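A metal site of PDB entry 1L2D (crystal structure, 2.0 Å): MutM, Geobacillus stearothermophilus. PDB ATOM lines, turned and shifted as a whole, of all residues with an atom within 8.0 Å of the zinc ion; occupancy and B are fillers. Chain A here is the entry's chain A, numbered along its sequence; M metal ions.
The side-chain sulfur (SG) of Cys 252 sits close to the side-chain hydroxyl (OG1) of Thr 254. SG of Cys 269 sits close to N of Arg 271, 3.6 Å away. The backbone NH (N) of Cys 269 is in hydrogen-bond range of the side-chain amide oxygen (OE1) of Gln 273 (2.9 Å). SG of Cys 249 sits close to N of Arg 251, 3.4 Å away. The backbone carbonyl oxygen of Thr 254 is in hydrogen-bond range of the backbone NH of Cys 249, 2.9 Å away.
Of the 18 residues printed, 4 come within 4 Å of the zinc ion. Along chain A the residues within 4 Å of the zinc ion span positions 249 to 272. The nearest printed residue that does not touch the zinc ion is Phe 182 (4.3 Å).
The zinc ion is bound by SG of Cys 272 (2.3 Å), SG of Cys 252 (2.4 Å), SG of Cys 269 (2.4 Å) and SG of Cys 249 (2.5 Å).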
ATOM      1  N   PHE A 182     -22.060  18.201 -18.329  1.00  0.00           N
ATOM      2  CA  PHE A 182     -21.067  17.405 -19.046  1.00  0.00           C
ATOM      3  C   PHE A 182     -20.755  16.140 -18.264  1.00  0.00           C
ATOM      4  O   PHE A 182     -20.797  15.037 -18.797  1.00  0.00           O
ATOM      5  CB  PHE A 182     -19.768  18.191 -19.240  1.00  0.00           C
ATOM      6  CG  PHE A 182     -18.613  17.334 -19.695  1.00  0.00           C
ATOM      7  CD1 PHE A 182     -18.466  16.988 -21.032  1.00  0.00           C
ATOM      8  CD2 PHE A 182     -17.720  16.807 -18.768  1.00  0.00           C
ATOM      9  CE1 PHE A 182     -17.458  16.122 -21.445  1.00  0.00           C
ATOM     10  CE2 PHE A 182     -16.703  15.942 -19.171  1.00  0.00           C
ATOM     11  CZ  PHE A 182     -16.566  15.595 -20.508  1.00  0.00           C
ATOM     12  N   TYR A 240     -13.939  20.874 -17.673  1.00  0.00           N
ATOM     13  CA  TYR A 240     -14.034  20.020 -18.845  1.00  0.00           C
ATOM     14  C   TYR A 240     -14.526  20.764 -20.081  1.00  0.00           C
ATOM     15  O   TYR A 240     -14.052  20.518 -21.192  1.00  0.00           O
ATOM     16  CB  TYR A 240     -14.986  18.856 -18.570  1.00  0.00           C
ATOM     17  CG  TYR A 240     -14.425  17.806 -17.642  1.00  0.00           C
ATOM     18  CD1 TYR A 240     -13.524  16.843 -18.111  1.00  0.00           C
ATOM     19  CD2 TYR A 240     -14.809  17.757 -16.301  1.00  0.00           C
ATOM     20  CE1 TYR A 240     -13.008  15.871 -17.258  1.00  0.00           C
ATOM     21  CE2 TYR A 240     -14.304  16.784 -15.440  1.00  0.00           C
ATOM     22  CZ  TYR A 240     -13.402  15.841 -15.928  1.00  0.00           C
ATOM     23  OH  TYR A 240     -12.905  14.868 -15.088  1.00  0.00           O
ATOM     24  N   VAL A 241     -15.457  21.706 -19.908  1.00  0.00           N
ATOM     25  CA  VAL A 241     -16.010  22.416 -21.051  1.00  0.00           C
ATOM     26  C   VAL A 241     -16.016  23.949 -21.054  1.00  0.00           C
ATOM     27  O   VAL A 241     -15.747  24.561 -22.091  1.00  0.00           O
ATOM     28  CB  VAL A 241     -17.454  21.924 -21.356  1.00  0.00           C
ATOM     29  CG1 VAL A 241     -17.435  20.433 -21.704  1.00  0.00           C
ATOM     30  CG2 VAL A 241     -18.354  22.143 -20.149  1.00  0.00           C
ATOM     31  N   PRO A 248      -9.788  20.032 -27.662  1.00  0.00           N
ATOM     32  CA  PRO A 248     -10.232  18.640 -27.534  1.00  0.00           C
ATOM     33  C   PRO A 248     -10.794  18.289 -26.159  1.00  0.00           C
ATOM     34  O   PRO A 248     -10.292  18.769 -25.130  1.00  0.00           O
ATOM     35  CB  PRO A 248      -8.975  17.840 -27.864  1.00  0.00           C
ATOM     36  CG  PRO A 248      -7.888  18.730 -27.339  1.00  0.00           C
ATOM     37  CD  PRO A 248      -8.317  20.097 -27.812  1.00  0.00           C
ATOM     38  N   CYS A 249     -11.845  17.470 -26.144  1.00  0.00           N
ATOM     39  CA  CYS A 249     -12.463  17.025 -24.909  1.00  0.00           C
ATOM     40  C   CYS A 249     -11.392  16.240 -24.143  1.00  0.00           C
ATOM     41  O   CYS A 249     -10.609  15.500 -24.746  1.00  0.00           O
ATOM     42  CB  CYS A 249     -13.661  16.108 -25.197  1.00  0.00           C
ATOM     43  SG  CYS A 249     -14.505  15.407 -23.732  1.00  0.00           S
ATOM     44  N   LYS A 250     -11.364  16.417 -22.827  1.00  0.00           N
ATOM     45  CA  LYS A 250     -10.388  15.725 -21.992  1.00  0.00           C
ATOM     46  C   LYS A 250     -10.701  14.232 -21.889  1.00  0.00           C
ATOM     47  O   LYS A 250      -9.825  13.435 -21.552  1.00  0.00           O
ATOM     48  CB  LYS A 250     -10.389  16.321 -20.573  1.00  0.00           C
ATOM     49  CG  LYS A 250      -9.916  17.774 -20.494  1.00  0.00           C
ATOM     50  CD  LYS A 250      -9.750  18.211 -19.045  1.00  0.00           C
ATOM     51  CE  LYS A 250      -9.309  19.672 -18.950  1.00  0.00           C
ATOM     52  NZ  LYS A 250      -8.993  20.068 -17.543  1.00  0.00           N
ATOM     53  N   ARG A 251     -11.929  13.864 -22.204  1.00  0.00           N
ATOM     54  CA  ARG A 251     -12.358  12.473 -22.115  1.00  0.00           C
ATOM     55  C   ARG A 251     -12.427  11.692 -23.445  1.00  0.00           C
ATOM     56  O   ARG A 251     -12.117  10.499 -23.459  1.00  0.00           O
ATOM     57  CB  ARG A 251     -13.728  12.423 -21.427  1.00  0.00           C
ATOM     58  CG  ARG A 251     -14.064  11.077 -20.831  1.00  0.00           C
ATOM     59  CD  ARG A 251     -14.623  11.236 -19.419  1.00  0.00           C
ATOM     60  NE  ARG A 251     -14.868   9.946 -18.771  1.00  0.00           N
ATOM     61  CZ  ARG A 251     -15.744   9.039 -19.208  1.00  0.00           C
ATOM     62  NH1 ARG A 251     -15.899   7.895 -18.546  1.00  0.00           N
ATOM     63  NH2 ARG A 251     -16.466   9.277 -20.288  1.00  0.00           N
ATOM     64  N   CYS A 252     -12.811  12.352 -24.536  1.00  0.00           N
ATOM     65  CA  CYS A 252     -12.901  11.649 -25.826  1.00  0.00           C
ATOM     66  C   CYS A 252     -12.115  12.295 -26.967  1.00  0.00           C
ATOM     67  O   CYS A 252     -11.967  11.687 -28.034  1.00  0.00           O
ATOM     68  CB  CYS A 252     -14.373  11.517 -26.251  1.00  0.00           C
ATOM     69  SG  CYS A 252     -15.117  13.044 -26.865  1.00  0.00           S
ATOM     70  N   GLY A 253     -11.633  13.518 -26.769  1.00  0.00           N
ATOM     71  CA  GLY A 253     -10.872  14.181 -27.811  1.00  0.00           C
ATOM     72  C   GLY A 253     -11.656  14.976 -28.842  1.00  0.00           C
ATOM     73  O   GLY A 253     -11.072  15.708 -29.645  1.00  0.00           O
ATOM     74  N   THR A 254     -12.979  14.832 -28.855  1.00  0.00           N
ATOM     75  CA  THR A 254     -13.823  15.572 -29.793  1.00  0.00           C
ATOM     76  C   THR A 254     -13.740  17.070 -29.462  1.00  0.00           C
ATOM     77  O   THR A 254     -13.776  17.444 -28.282  1.00  0.00           O
ATOM     78  CB  THR A 254     -15.294  15.127 -29.687  1.00  0.00           C
ATOM     79  OG1 THR A 254     -15.418  13.758 -30.082  1.00  0.00           O
ATOM     80  CG2 THR A 254     -16.183  15.995 -30.579  1.00  0.00           C
ATOM     81  N   PRO A 255     -13.650  17.941 -30.489  1.00  0.00           N
ATOM     82  CA  PRO A 255     -13.565  19.378 -30.218  1.00  0.00           C
ATOM     83  C   PRO A 255     -14.762  19.910 -29.440  1.00  0.00           C
ATOM     84  O   PRO A 255     -15.911  19.627 -29.785  1.00  0.00           O
ATOM     85  CB  PRO A 255     -13.481  19.990 -31.622  1.00  0.00           C
ATOM     86  CG  PRO A 255     -12.885  18.878 -32.465  1.00  0.00           C
ATOM     87  CD  PRO A 255     -13.616  17.667 -31.929  1.00  0.00           C
ATOM     88  N   ILE A 256     -14.504  20.684 -28.389  1.00  0.00           N
ATOM     89  CA  ILE A 256     -15.565  21.265 -27.592  1.00  0.00           C
ATOM     90  C   ILE A 256     -16.254  22.346 -28.415  1.00  0.00           C
ATOM     91  O   ILE A 256     -15.593  23.112 -29.127  1.00  0.00           O
ATOM     92  CB  ILE A 256     -15.008  21.877 -26.282  1.00  0.00           C
ATOM     93  CG1 ILE A 256     -14.384  20.782 -25.417  1.00  0.00           C
ATOM     94  CG2 ILE A 256     -16.113  22.616 -25.530  1.00  0.00           C
ATOM     95  CD1 ILE A 256     -15.325  19.608 -25.150  1.00  0.00           C
ATOM     96  N   TYR A 268     -20.196  22.581 -24.428  1.00  0.00           N
ATOM     97  CA  TYR A 268     -20.493  21.148 -24.322  1.00  0.00           C
ATOM     98  C   TYR A 268     -19.729  20.289 -25.342  1.00  0.00           C
ATOM     99  O   TYR A 268     -19.169  20.789 -26.312  1.00  0.00           O
ATOM    100  CB  TYR A 268     -21.994  20.933 -24.560  1.00  0.00           C
ATOM    101  CG  TYR A 268     -22.408  21.202 -26.003  1.00  0.00           C
ATOM    102  CD1 TYR A 268     -22.579  20.152 -26.895  1.00  0.00           C
ATOM    103  CD2 TYR A 268     -22.561  22.506 -26.471  1.00  0.00           C
ATOM    104  CE1 TYR A 268     -22.893  20.387 -28.234  1.00  0.00           C
ATOM    105  CE2 TYR A 268     -22.877  22.751 -27.810  1.00  0.00           C
ATOM    106  CZ  TYR A 268     -23.039  21.692 -28.681  1.00  0.00           C
ATOM    107  OH  TYR A 268     -23.324  21.919 -30.007  1.00  0.00           O
ATOM    108  N   CYS A 269     -19.717  18.976 -25.104  1.00  0.00           N
ATOM    109  CA  CYS A 269     -19.072  18.029 -26.020  1.00  0.00           C
ATOM    110  C   CYS A 269     -20.197  17.257 -26.700  1.00  0.00           C
ATOM    111  O   CYS A 269     -21.000  16.602 -26.035  1.00  0.00           O
ATOM    112  CB  CYS A 269     -18.180  17.041 -25.250  1.00  0.00           C
ATOM    113  SG  CYS A 269     -17.491  15.706 -26.315  1.00  0.00           S
ATOM    114  N   PRO A 270     -20.278  17.327 -28.041  1.00  0.00           N
ATOM    115  CA  PRO A 270     -21.326  16.621 -28.801  1.00  0.00           C
ATOM    116  C   PRO A 270     -21.322  15.098 -28.707  1.00  0.00           C
ATOM    117  O   PRO A 270     -22.335  14.453 -28.998  1.00  0.00           O
ATOM    118  CB  PRO A 270     -21.111  17.131 -30.229  1.00  0.00           C
ATOM    119  CG  PRO A 270     -19.644  17.356 -30.277  1.00  0.00           C
ATOM    120  CD  PRO A 270     -19.365  18.030 -28.952  1.00  0.00           C
ATOM    121  N   ARG A 271     -20.197  14.517 -28.295  1.00  0.00           N
ATOM    122  CA  ARG A 271     -20.122  13.059 -28.162  1.00  0.00           C
ATOM    123  C   ARG A 271     -20.428  12.573 -26.745  1.00  0.00           C
ATOM    124  O   ARG A 271     -21.243  11.669 -26.569  1.00  0.00           O
ATOM    125  CB  ARG A 271     -18.738  12.528 -28.593  1.00  0.00           C
ATOM    126  CG  ARG A 271     -18.582  11.014 -28.358  1.00  0.00           C
ATOM    127  CD  ARG A 271     -17.258  10.429 -28.849  1.00  0.00           C
ATOM    128  NE  ARG A 271     -17.230   8.977 -28.660  1.00  0.00           N
ATOM    129  CZ  ARG A 271     -16.271   8.158 -29.110  1.00  0.00           C
ATOM    130  NH1 ARG A 271     -16.368   6.849 -28.886  1.00  0.00           N
ATOM    131  NH2 ARG A 271     -15.226   8.648 -29.765  1.00  0.00           N
ATOM    132  N   CYS A 272     -19.779  13.162 -25.736  1.00  0.00           N
ATOM    133  CA  CYS A 272     -20.005  12.742 -24.348  1.00  0.00           C
ATOM    134  C   CYS A 272     -21.408  13.081 -23.831  1.00  0.00           C
ATOM    135  O   CYS A 272     -21.929  12.374 -22.979  1.00  0.00           O
ATOM    136  CB  CYS A 272     -18.966  13.397 -23.418  1.00  0.00           C
ATOM    137  SG  CYS A 272     -17.269  12.765 -23.568  1.00  0.00           S
ATOM    138  N   GLN A 273     -21.993  14.148 -24.358  1.00  0.00           N
ATOM    139  CA  GLN A 273     -23.328  14.572 -23.942  1.00  0.00           C
ATOM    140  C   GLN A 273     -24.406  14.226 -24.954  1.00  0.00           C
ATOM    141  O   GLN A 273     -24.281  14.529 -26.134  1.00  0.00           O
ATOM    142  CB  GLN A 273     -23.329  16.084 -23.662  1.00  0.00           C
ATOM    143  CG  GLN A 273     -22.624  16.455 -22.356  1.00  0.00           C
ATOM    144  CD  GLN A 273     -22.320  17.938 -22.238  1.00  0.00           C
ATOM    145  OE1 GLN A 273     -21.270  18.407 -22.691  1.00  0.00           O
ATOM    146  NE2 GLN A 273     -23.243  18.698 -21.653  1.00  0.00           N
HETATM  147 ZN    ZN M   1     -16.186  14.152 -25.024  1.00  0.00          ZN
